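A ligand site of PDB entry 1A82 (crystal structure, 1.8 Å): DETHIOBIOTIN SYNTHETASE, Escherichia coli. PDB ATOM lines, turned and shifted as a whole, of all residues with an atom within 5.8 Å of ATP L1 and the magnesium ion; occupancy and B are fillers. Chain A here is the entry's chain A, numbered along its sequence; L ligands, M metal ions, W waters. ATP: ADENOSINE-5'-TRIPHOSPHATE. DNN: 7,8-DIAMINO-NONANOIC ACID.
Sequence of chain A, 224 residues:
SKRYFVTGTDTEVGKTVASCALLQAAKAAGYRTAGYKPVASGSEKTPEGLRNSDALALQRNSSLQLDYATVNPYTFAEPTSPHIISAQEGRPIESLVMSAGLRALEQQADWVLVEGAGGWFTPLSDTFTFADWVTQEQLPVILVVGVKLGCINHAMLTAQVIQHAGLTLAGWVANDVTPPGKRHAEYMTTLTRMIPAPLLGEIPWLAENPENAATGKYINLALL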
ATOM      1  N   ASP A  10      17.085 -28.694  25.069  1.00  0.00           N
ATOM      2  CA  ASP A  10      17.745 -30.001  25.078  1.00  0.00           C
ATOM      3  C   ASP A  10      19.203 -29.748  25.514  1.00  0.00           C
ATOM      4  O   ASP A  10      19.569 -28.629  25.868  1.00  0.00           O
ATOM      5  CB  ASP A  10      17.752 -30.540  23.637  1.00  0.00           C
ATOM      6  CG  ASP A  10      18.124 -32.029  23.532  1.00  0.00           C
ATOM      7  OD1 ASP A  10      18.335 -32.715  24.560  1.00  0.00           O
ATOM      8  OD2 ASP A  10      18.174 -32.502  22.380  1.00  0.00           O
ATOM      9  N   THR A  11      20.009 -30.798  25.537  1.00  0.00           N
ATOM     10  CA  THR A  11      21.426 -30.660  25.815  1.00  0.00           C
ATOM     11  C   THR A  11      21.999 -30.282  24.426  1.00  0.00           C
ATOM     12  O   THR A  11      21.363 -30.551  23.403  1.00  0.00           O
ATOM     13  CB  THR A  11      22.050 -31.994  26.353  1.00  0.00           C
ATOM     14  OG1 THR A  11      23.450 -31.800  26.610  1.00  0.00           O
ATOM     15  CG2 THR A  11      21.856 -33.147  25.352  1.00  0.00           C
ATOM     16  N   GLU A  12      23.129 -29.595  24.403  1.00  0.00           N
ATOM     17  CA  GLU A  12      23.772 -29.198  23.141  1.00  0.00           C
ATOM     18  C   GLU A  12      22.951 -28.265  22.238  1.00  0.00           C
ATOM     19  O   GLU A  12      22.964 -28.408  21.029  1.00  0.00           O
ATOM     20  CB  GLU A  12      24.197 -30.428  22.324  1.00  0.00           C
ATOM     21  CG  GLU A  12      25.699 -30.494  22.050  1.00  0.00           C
ATOM     22  CD  GLU A  12      26.513 -30.897  23.284  1.00  0.00           C
ATOM     23  OE1 GLU A  12      26.155 -30.485  24.420  1.00  0.00           O
ATOM     24  OE2 GLU A  12      27.503 -31.645  23.126  1.00  0.00           O
ATOM     25  N   VAL A  13      22.236 -27.304  22.824  1.00  0.00           N
ATOM     26  CA  VAL A  13      21.480 -26.356  22.011  1.00  0.00           C
ATOM     27  C   VAL A  13      22.063 -24.961  22.136  1.00  0.00           C
ATOM     28  O   VAL A  13      21.613 -24.030  21.444  1.00  0.00           O
ATOM     29  CB  VAL A  13      19.982 -26.338  22.386  1.00  0.00           C
ATOM     30  CG1 VAL A  13      19.369 -27.702  22.119  1.00  0.00           C
ATOM     31  CG2 VAL A  13      19.777 -25.930  23.837  1.00  0.00           C
ATOM     32  N   GLY A  14      23.032 -24.799  23.037  1.00  0.00           N
ATOM     33  CA  GLY A  14      23.689 -23.517  23.224  1.00  0.00           C
ATOM     34  C   GLY A  14      23.529 -22.825  24.573  1.00  0.00           C
ATOM     35  O   GLY A  14      23.772 -21.622  24.652  1.00  0.00           O
ATOM     36  N   LYS A  15      23.123 -23.540  25.617  1.00  0.00           N
ATOM     37  CA  LYS A  15      22.997 -22.918  26.949  1.00  0.00           C
ATOM     38  C   LYS A  15      24.286 -22.185  27.344  1.00  0.00           C
ATOM     39  O   LYS A  15      24.235 -21.059  27.815  1.00  0.00           O
ATOM     40  CB  LYS A  15      22.665 -23.953  28.041  1.00  0.00           C
ATOM     41  CG  LYS A  15      21.269 -24.602  27.938  1.00  0.00           C
ATOM     42  CD  LYS A  15      20.975 -25.467  29.167  1.00  0.00           C
ATOM     43  CE  LYS A  15      21.969 -26.567  29.322  1.00  0.00           C
ATOM     44  NZ  LYS A  15      21.871 -27.509  28.159  1.00  0.00           N
ATOM     45  N   THR A  16      25.429 -22.830  27.129  1.00  0.00           N
ATOM     46  CA  THR A  16      26.720 -22.232  27.507  1.00  0.00           C
ATOM     47  C   THR A  16      27.069 -21.001  26.676  1.00  0.00           C
ATOM     48  O   THR A  16      27.444 -19.967  27.229  1.00  0.00           O
ATOM     49  CB  THR A  16      27.864 -23.303  27.496  1.00  0.00           C
ATOM     50  OG1 THR A  16      27.575 -24.280  28.510  1.00  0.00           O
ATOM     51  CG2 THR A  16      29.236 -22.680  27.788  1.00  0.00           C
ATOM     52  N   VAL A  17      26.921 -21.082  25.364  1.00  0.00           N
ATOM     53  CA  VAL A  17      27.205 -19.941  24.500  1.00  0.00           C
ATOM     54  C   VAL A  17      26.276 -18.756  24.880  1.00  0.00           C
ATOM     55  O   VAL A  17      26.745 -17.623  25.032  1.00  0.00           O
ATOM     56  CB  VAL A  17      27.071 -20.318  22.996  1.00  0.00           C
ATOM     57  CG1 VAL A  17      26.996 -19.053  22.104  1.00  0.00           C
ATOM     58  CG2 VAL A  17      28.266 -21.149  22.566  1.00  0.00           C
ATOM     59  N   ALA A  18      24.985 -19.012  25.017  1.00  0.00           N
ATOM     60  CA  ALA A  18      24.050 -17.959  25.385  1.00  0.00           C
ATOM     61  C   ALA A  18      24.358 -17.407  26.769  1.00  0.00           C
ATOM     62  O   ALA A  18      24.245 -16.201  26.977  1.00  0.00           O
ATOM     63  CB  ALA A  18      22.628 -18.453  25.328  1.00  0.00           C
ATOM     64  N   LYS A  37      27.607 -23.077  37.649  1.00  0.00           N
ATOM     65  CA  LYS A  37      27.288 -24.366  37.006  1.00  0.00           C
ATOM     66  C   LYS A  37      27.404 -25.369  38.168  1.00  0.00           C
ATOM     67  O   LYS A  37      28.398 -26.081  38.276  1.00  0.00           O
ATOM     68  CB  LYS A  37      28.339 -24.663  35.906  1.00  0.00           C
ATOM     69  CG  LYS A  37      28.192 -26.004  35.167  1.00  0.00           C
ATOM     70  CD  LYS A  37      27.080 -25.997  34.102  1.00  0.00           C
ATOM     71  CE  LYS A  37      27.019 -27.347  33.358  1.00  0.00           C
ATOM     72  NZ  LYS A  37      26.030 -27.309  32.223  1.00  0.00           N
ATOM     73  N   ASP A  54      32.113 -25.993  30.395  1.00  0.00           N
ATOM     74  CA  ASP A  54      31.027 -25.030  30.625  1.00  0.00           C
ATOM     75  C   ASP A  54      31.404 -24.168  31.832  1.00  0.00           C
ATOM     76  O   ASP A  54      31.297 -22.949  31.817  1.00  0.00           O
ATOM     77  CB  ASP A  54      29.716 -25.739  30.982  1.00  0.00           C
ATOM     78  CG  ASP A  54      29.088 -26.469  29.813  1.00  0.00           C
ATOM     79  OD1 ASP A  54      29.761 -26.696  28.793  1.00  0.00           O
ATOM     80  OD2 ASP A  54      27.880 -26.802  29.933  1.00  0.00           O
ATOM     81  N   GLU A 115      23.676 -21.953  35.070  1.00  0.00           N
ATOM     82  CA  GLU A 115      23.410 -22.840  33.926  1.00  0.00           C
ATOM     83  C   GLU A 115      23.046 -24.238  34.455  1.00  0.00           C
ATOM     84  O   GLU A 115      23.684 -24.742  35.381  1.00  0.00           O
ATOM     85  CB  GLU A 115      24.591 -22.926  32.947  1.00  0.00           C
ATOM     86  CG  GLU A 115      24.250 -23.789  31.735  1.00  0.00           C
ATOM     87  CD  GLU A 115      25.434 -24.140  30.847  1.00  0.00           C
ATOM     88  OE1 GLU A 115      26.462 -23.420  30.864  1.00  0.00           O
ATOM     89  OE2 GLU A 115      25.317 -25.151  30.101  1.00  0.00           O
ATOM     90  N   GLY A 116      21.967 -24.801  33.922  1.00  0.00           N
ATOM     91  CA  GLY A 116      21.541 -26.117  34.332  1.00  0.00           C
ATOM     92  C   GLY A 116      22.395 -27.129  33.595  1.00  0.00           C
ATOM     93  O   GLY A 116      23.479 -26.800  33.134  1.00  0.00           O
ATOM     94  N   ALA A 117      21.914 -28.361  33.494  1.00  0.00           N
ATOM     95  CA  ALA A 117      22.641 -29.409  32.790  1.00  0.00           C
ATOM     96  C   ALA A 117      21.587 -30.089  31.940  1.00  0.00           C
ATOM     97  O   ALA A 117      20.485 -30.381  32.416  1.00  0.00           O
ATOM     98  CB  ALA A 117      23.277 -30.403  33.777  1.00  0.00           C
ATOM     99  N   GLY A 118      21.898 -30.289  30.662  1.00  0.00           N
ATOM    100  CA  GLY A 118      20.905 -30.903  29.783  1.00  0.00           C
ATOM    101  C   GLY A 118      19.661 -30.027  29.655  1.00  0.00           C
ATOM    102  O   GLY A 118      19.751 -28.797  29.507  1.00  0.00           O
ATOM    103  N   GLY A 119      18.502 -30.651  29.736  1.00  0.00           N
ATOM    104  CA  GLY A 119      17.252 -29.931  29.620  1.00  0.00           C
ATOM    105  C   GLY A 119      16.610 -29.726  30.976  1.00  0.00           C
ATOM    106  O   GLY A 119      17.216 -30.032  32.007  1.00  0.00           O
ATOM    107  N   ASN A 175      19.291 -19.157  19.549  1.00  0.00           N
ATOM    108  CA  ASN A 175      20.680 -19.433  19.238  1.00  0.00           C
ATOM    109  C   ASN A 175      20.813 -20.145  17.895  1.00  0.00           C
ATOM    110  O   ASN A 175      20.242 -21.214  17.695  1.00  0.00           O
ATOM    111  CB  ASN A 175      21.314 -20.264  20.346  1.00  0.00           C
ATOM    112  CG  ASN A 175      22.788 -20.498  20.110  1.00  0.00           C
ATOM    113  OD1 ASN A 175      23.498 -19.578  19.755  1.00  0.00           O
ATOM    114  ND2 ASN A 175      23.249 -21.724  20.299  1.00  0.00           N
ATOM    115  N   ASP A 176      21.545 -19.536  16.962  1.00  0.00           N
ATOM    116  CA  ASP A 176      21.718 -20.120  15.642  1.00  0.00           C
ATOM    117  C   ASP A 176      22.814 -21.156  15.674  1.00  0.00           C
ATOM    118  O   ASP A 176      23.998 -20.858  15.490  1.00  0.00           O
ATOM    119  CB  ASP A 176      22.022 -19.031  14.610  1.00  0.00           C
ATOM    120  CG  ASP A 176      20.945 -17.955  14.572  1.00  0.00           C
ATOM    121  OD1 ASP A 176      19.861 -18.154  15.151  1.00  0.00           O
ATOM    122  OD2 ASP A 176      21.192 -16.891  13.962  1.00  0.00           O
ATOM    123  N   VAL A 177      22.419 -22.388  15.935  1.00  0.00           N
ATOM    124  CA  VAL A 177      23.346 -23.493  16.025  1.00  0.00           C
ATOM    125  C   VAL A 177      23.942 -23.881  14.673  1.00  0.00           C
ATOM    126  O   VAL A 177      25.037 -24.448  14.614  1.00  0.00           O
ATOM    127  CB  VAL A 177      22.714 -24.726  16.736  1.00  0.00           C
ATOM    128  CG1 VAL A 177      22.521 -24.438  18.210  1.00  0.00           C
ATOM    129  CG2 VAL A 177      21.377 -25.067  16.138  1.00  0.00           C
ATOM    130  N   ILE A 203      21.720 -15.058  18.912  1.00  0.00           N
ATOM    131  CA  ILE A 203      23.151 -15.211  18.725  1.00  0.00           C
ATOM    132  C   ILE A 203      23.380 -15.829  17.339  1.00  0.00           C
ATOM    133  O   ILE A 203      22.830 -16.881  17.013  1.00  0.00           O
ATOM    134  CB  ILE A 203      23.743 -16.069  19.854  1.00  0.00           C
ATOM    135  CG1 ILE A 203      23.531 -15.331  21.190  1.00  0.00           C
ATOM    136  CG2 ILE A 203      25.236 -16.377  19.617  1.00  0.00           C
ATOM    137  CD1 ILE A 203      23.973 -16.102  22.366  1.00  0.00           C
ATOM    138  N   PRO A 204      24.138 -15.134  16.490  1.00  0.00           N
ATOM    139  CA  PRO A 204      24.421 -15.632  15.131  1.00  0.00           C
ATOM    140  C   PRO A 204      25.215 -16.924  15.137  1.00  0.00           C
ATOM    141  O   PRO A 204      25.798 -17.307  16.164  1.00  0.00           O
ATOM    142  CB  PRO A 204      25.269 -14.508  14.507  1.00  0.00           C
ATOM    143  CG  PRO A 204      24.979 -13.305  15.353  1.00  0.00           C
ATOM    144  CD  PRO A 204      24.813 -13.843  16.728  1.00  0.00           C
ATOM    145  N   TRP A 205      25.256 -17.589  13.987  1.00  0.00           N
ATOM    146  CA  TRP A 205      26.041 -18.823  13.835  1.00  0.00           C
ATOM    147  C   TRP A 205      27.506 -18.397  13.821  1.00  0.00           C
ATOM    148  O   TRP A 205      27.970 -17.781  12.850  1.00  0.00           O
ATOM    149  CB  TRP A 205      25.675 -19.559  12.536  1.00  0.00           C
ATOM    150  CG  TRP A 205      26.576 -20.718  12.259  1.00  0.00           C
ATOM    151  CD1 TRP A 205      26.737 -21.858  13.021  1.00  0.00           C
ATOM    152  CD2 TRP A 205      27.502 -20.828  11.185  1.00  0.00           C
ATOM    153  NE1 TRP A 205      27.710 -22.666  12.474  1.00  0.00           N
ATOM    154  CE2 TRP A 205      28.198 -22.057  11.341  1.00  0.00           C
ATOM    155  CE3 TRP A 205      27.812 -20.009  10.088  1.00  0.00           C
ATOM    156  CZ2 TRP A 205      29.196 -22.478  10.456  1.00  0.00           C
ATOM    157  CZ3 TRP A 205      28.809 -20.430   9.203  1.00  0.00           C
ATOM    158  CH2 TRP A 205      29.482 -21.647   9.390  1.00  0.00           C
ATOM    159  N   LEU A 206      28.219 -18.662  14.921  1.00  0.00           N
ATOM    160  CA  LEU A 206      29.622 -18.302  15.079  1.00  0.00           C
ATOM    161  C   LEU A 206      30.459 -19.569  15.177  1.00  0.00           C
ATOM    162  O   LEU A 206      30.708 -20.117  16.255  1.00  0.00           O
ATOM    163  CB  LEU A 206      29.798 -17.432  16.328  1.00  0.00           C
ATOM    164  CG  LEU A 206      29.143 -16.057  16.158  1.00  0.00           C
ATOM    165  CD1 LEU A 206      28.672 -15.499  17.495  1.00  0.00           C
ATOM    166  CD2 LEU A 206      30.118 -15.120  15.478  1.00  0.00           C
ATOM    167  N   ALA A 207      30.865 -20.053  14.012  1.00  0.00           N
ATOM    168  CA  ALA A 207      31.628 -21.291  13.882  1.00  0.00           C
ATOM    169  C   ALA A 207      32.807 -21.496  14.837  1.00  0.00           C
ATOM    170  O   ALA A 207      32.879 -22.515  15.532  1.00  0.00           O
ATOM    171  CB  ALA A 207      32.074 -21.462  12.437  1.00  0.00           C
ATOM    172  N   PRO A 210      32.719 -19.752  19.726  1.00  0.00           N
ATOM    173  CA  PRO A 210      31.655 -18.809  20.102  1.00  0.00           C
ATOM    174  C   PRO A 210      31.552 -18.489  21.593  1.00  0.00           C
ATOM    175  O   PRO A 210      30.926 -17.515  21.976  1.00  0.00           O
ATOM    176  CB  PRO A 210      30.392 -19.479  19.556  1.00  0.00           C
ATOM    177  CG  PRO A 210      30.713 -20.941  19.701  1.00  0.00           C
ATOM    178  CD  PRO A 210      32.149 -21.016  19.236  1.00  0.00           C
ATOM    179  N   GLU A 211      32.179 -19.314  22.433  1.00  0.00           N
ATOM    180  CA  GLU A 211      32.163 -19.101  23.888  1.00  0.00           C
ATOM    181  C   GLU A 211      33.030 -17.889  24.209  1.00  0.00           C
ATOM    182  O   GLU A 211      32.818 -17.207  25.225  1.00  0.00           O
ATOM    183  CB  GLU A 211      32.712 -20.332  24.654  1.00  0.00           C
ATOM    184  CG  GLU A 211      31.864 -21.600  24.552  1.00  0.00           C
ATOM    185  CD  GLU A 211      32.012 -22.348  23.223  1.00  0.00           C
ATOM    186  OE1 GLU A 211      32.961 -22.076  22.455  1.00  0.00           O
ATOM    187  OE2 GLU A 211      31.174 -23.230  22.925  1.00  0.00           O
HETATM  188  PG  ATP L   1      25.159 -29.004  27.679  1.00  0.00           P
HETATM  189  O1G ATP L   1      26.392 -29.849  27.605  1.00  0.00           O
HETATM  190  O2G ATP L   1      23.812 -29.642  27.969  1.00  0.00           O
HETATM  191  O3G ATP L   1      25.297 -27.966  28.922  1.00  0.00           O
HETATM  192  PB  ATP L   1      24.714 -26.616  25.856  1.00  0.00           P
HETATM  193  O1B ATP L   1      25.423 -25.792  26.868  1.00  0.00           O
HETATM  194  O2B ATP L   1      23.239 -26.512  25.717  1.00  0.00           O
HETATM  195  O3B ATP L   1      25.077 -28.139  26.201  1.00  0.00           O
HETATM  196  PA  ATP L   1      26.737 -25.349  24.091  1.00  0.00           P
HETATM  197  O1A ATP L   1      26.586 -23.878  24.327  1.00  0.00           O
HETATM  198  O2A ATP L   1      27.884 -26.074  24.662  1.00  0.00           O
HETATM  199  O3A ATP L   1      25.356 -26.117  24.496  1.00  0.00           O
HETATM  200  O5' ATP L   1      26.648 -25.548  22.487  1.00  0.00           O
HETATM  201  C5' ATP L   1      26.773 -26.874  21.930  1.00  0.00           C
HETATM  202  C4' ATP L   1      27.781 -26.881  20.779  1.00  0.00           C
HETATM  203  O4' ATP L   1      27.348 -26.066  19.663  1.00  0.00           O
HETATM  204  C3' ATP L   1      29.186 -26.416  21.162  1.00  0.00           C
HETATM  205  O3' ATP L   1      30.245 -27.117  20.493  1.00  0.00           O
HETATM  206  C2' ATP L   1      29.165 -24.951  20.737  1.00  0.00           C
HETATM  207  O2' ATP L   1      30.496 -24.452  20.505  1.00  0.00           O
HETATM  208  C1' ATP L   1      28.287 -25.003  19.493  1.00  0.00           C
HETATM  209  N9  ATP L   1      27.515 -23.731  19.375  1.00  0.00           N
HETATM  210  C8  ATP L   1      26.643 -23.288  20.277  1.00  0.00           C
HETATM  211  N7  ATP L   1      26.156 -22.116  19.863  1.00  0.00           N
HETATM  212  C5  ATP L   1      26.714 -21.817  18.692  1.00  0.00           C
HETATM  213  C6  ATP L   1      26.600 -20.750  17.817  1.00  0.00           C
HETATM  214  N6  ATP L   1      25.800 -19.715  18.066  1.00  0.00           N
HETATM  215  N1  ATP L   1      27.338 -20.768  16.694  1.00  0.00           N
HETATM  216  C2  ATP L   1      28.160 -21.789  16.420  1.00  0.00           C
HETATM  217  N3  ATP L   1      28.282 -22.822  17.244  1.00  0.00           N
HETATM  218  C4  ATP L   1      27.575 -22.854  18.373  1.00  0.00           C
HETATM  219  C1  DNN L   2      18.604 -36.453  29.699  1.00  0.00           C
HETATM  220  O1  DNN L   2      17.561 -35.779  29.609  1.00  0.00           O
HETATM  221  O2  DNN L   2      18.723 -37.578  29.166  1.00  0.00           O
HETATM  222  C2  DNN L   2      19.752 -35.881  30.507  1.00  0.00           C
HETATM  223  C3  DNN L   2      20.939 -35.464  29.643  1.00  0.00           C
HETATM  224  C4  DNN L   2      21.898 -34.526  30.391  1.00  0.00           C
HETATM  225  C5  DNN L   2      23.164 -34.316  29.595  1.00  0.00           C
HETATM  226  C6  DNN L   2      23.975 -33.079  30.016  1.00  0.00           C
HETATM  227  C7  DNN L   2      25.498 -33.275  29.876  1.00  0.00           C
HETATM  228  C8  DNN L   2      25.861 -33.739  28.458  1.00  0.00           C
HETATM  229  C9  DNN L   2      26.777 -34.911  28.572  1.00  0.00           C
HETATM  230  N7  DNN L   2      26.281 -32.096  30.346  1.00  0.00           N
HETATM  231  N8  DNN L   2      26.489 -32.662  27.615  1.00  0.00           N
HETATM  232 MG    MG M   1      26.353 -26.087  28.579  1.00  0.00          MG
HETATM  233  O   HOH W   1      30.605 -24.386  16.593  1.00  0.00           O
HETATM  234  O   HOH W   2      32.196 -25.326  18.452  1.00  0.00           O
HETATM  235  O   HOH W   3      33.882 -24.273  20.916  1.00  0.00           O
HETATM  236  O   HOH W   4      24.991 -29.707  30.552  1.00  0.00           O
HETATM  237  O   HOH W   5      30.364 -25.156  24.743  1.00  0.00           O
HETATM  238  O   HOH W   6      28.720 -29.792  29.938  1.00  0.00           O
HETATM  239  O   HOH W   7      27.824 -27.159  27.020  1.00  0.00           O
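Water W7 lies within hydrogen-bond range of an oxygen (O2A) of ATP L1 (2.6 Å) and the side-chain carboxylate of Asp 54 (2.7 Å).
Water W4 lies within hydrogen-bond range of N7 of DNN L2, O2G of ATP L1, NZ of Lys 37 and N of Gly 118.
Water W5 bridges an oxygen (O2A) of ATP L1 (2.6 Å) and the side-chain carboxylate of Glu 211 (2.8 Å).
Water W1 bridges N3 of ATP L1 and O of Ala 207.
Water W6 lies within hydrogen-bond range of O1G of ATP L1 (3.3 Å), N7 of DNN L2 (3.4 Å) and OD1 of Asp 54 (3.5 Å).
Water W3 bridges OE1 of Glu 211 (2.8 Å) and O2' of ATP L1 (3.4 Å).
The backbone NH (N) of Thr 16 is in hydrogen-bond range of an oxygen (O1A) of ATP L1 (3.2 Å).
An oxygen (O2B) of ATP L1 lies within hydrogen-bond range of the backbone NH (N) of Val 13 (3.2 Å).
The backbone NH (N) of Lys 15 sits at hydrogen-bond distance from an oxygen (O2B) of ATP L1, at 3.0 Å.
The backbone NH (N) of Gly 118 lies within hydrogen-bond range of an oxygen (O2G) of ATP L1.
The side-chain amino group of Lys 37 lies close to an oxygen (O3G) of ATP L1 (3.4 Å).
The backbone NH of Gly 14 lies within hydrogen-bond range of an oxygen (O3A) of ATP L1 (3.0 Å).
OD1 of Asn 175 sits at hydrogen-bond distance from N6 of ATP L1 (2.9 Å).
The backbone NH of Leu 206 sits at hydrogen-bond distance from a nitrogen (N1) of ATP L1, at 2.9 Å.
The side-chain carboxylate (OE2) of Glu 211 lies within hydrogen-bond range of an oxygen (O2') of ATP L1, at 2.8 Å.
The backbone NH (N) of Val 17 is in hydrogen-bond range of an oxygen (O1A) of ATP L1.
An oxygen (O3B) of ATP L1 sits at hydrogen-bond distance from the backbone NH (N) of Glu 12 (3.0 Å).
OG1 of Thr 11 is in hydrogen-bond range of O2G of ATP L1 (2.6 Å).
The side-chain hydroxyl of Thr 11 lies within hydrogen-bond range of a nitrogen (N8) of DNN L2, at 3.3 Å.
A nitrogen (N6) of ATP L1 is in hydrogen-bond range of the backbone carbonyl oxygen of Asp 176 (3.3 Å).
O2G of ATP L1 lies within salt-bridge range of NZ of Lys 15.
The side-chain carboxylate (OE1) of Glu 12 is in salt-bridge range of a nitrogen (N8) of DNN L2 (3.9 Å).
O of Pro 204 sits at hydrogen-bond distance from N6 of ATP L1 (3.1 Å).
An oxygen (O1G) of ATP L1 lies within hydrogen-bond range of a nitrogen (N8) of DNN L2 (2.8 Å).
NZ of Lys 37 sits close to OE2 of Glu 115.
The side-chain amino group of Lys 15 lies within hydrogen-bond range of the backbone carbonyl oxygen of Asp 10 (3.4 Å).
The backbone carbonyl oxygen (O) of Ile 203 lies within hydrogen-bond range of the backbone NH (N) of Asp 176, at 3.0 Å.
The side-chain amino group (NZ) of Lys 37 lies within hydrogen-bond range of the backbone carbonyl oxygen (O) of Gly 116, 2.8 Å away.
The side-chain amide nitrogen (ND2) of Asn 175 sits at hydrogen-bond distance from the backbone carbonyl oxygen (O) of Val 13 (3.1 Å).
The side-chain amino group (NZ) of Lys 15 is in hydrogen-bond range of the backbone carbonyl oxygen (O) of Gly 118, at 2.8 Å.
OD2 of Asp 54 lies close to NZ of Lys 37 (3.0 Å).
O1B of ATP L1 binds the magnesium ion (2.0 Å).
The side-chain carboxylate (OE2) of Glu 115 is bound to the magnesium ion (2.1 Å).
OD2 of Asp 54 binds the magnesium ion, at 2.2 Å.
The magnesium ion is bound by OG1 of Thr 16 (2.2 Å).
O3G of ATP L1 binds the magnesium ion, 2.2 Å away.
The magnesium ion is bound by water W7 (2.4 Å).
Residues that only touch the magnesium ion: Lys 37.
The nearest printed residue that does not touch the magnesium ion is Lys 15 (4.3 Å).
Ile 203 touches ATP L1.
Trp 205 touches ATP L1.
Pro 210 touches ATP L1.
Hydrophobic or aromatic side chains within 4 Å of ATP L1: Val 13, Val 17, Ile 203, Trp 205 and Pro 210.
The nearest printed residue that does not touch ATP L1 is Ala 207 (4.02 Å).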
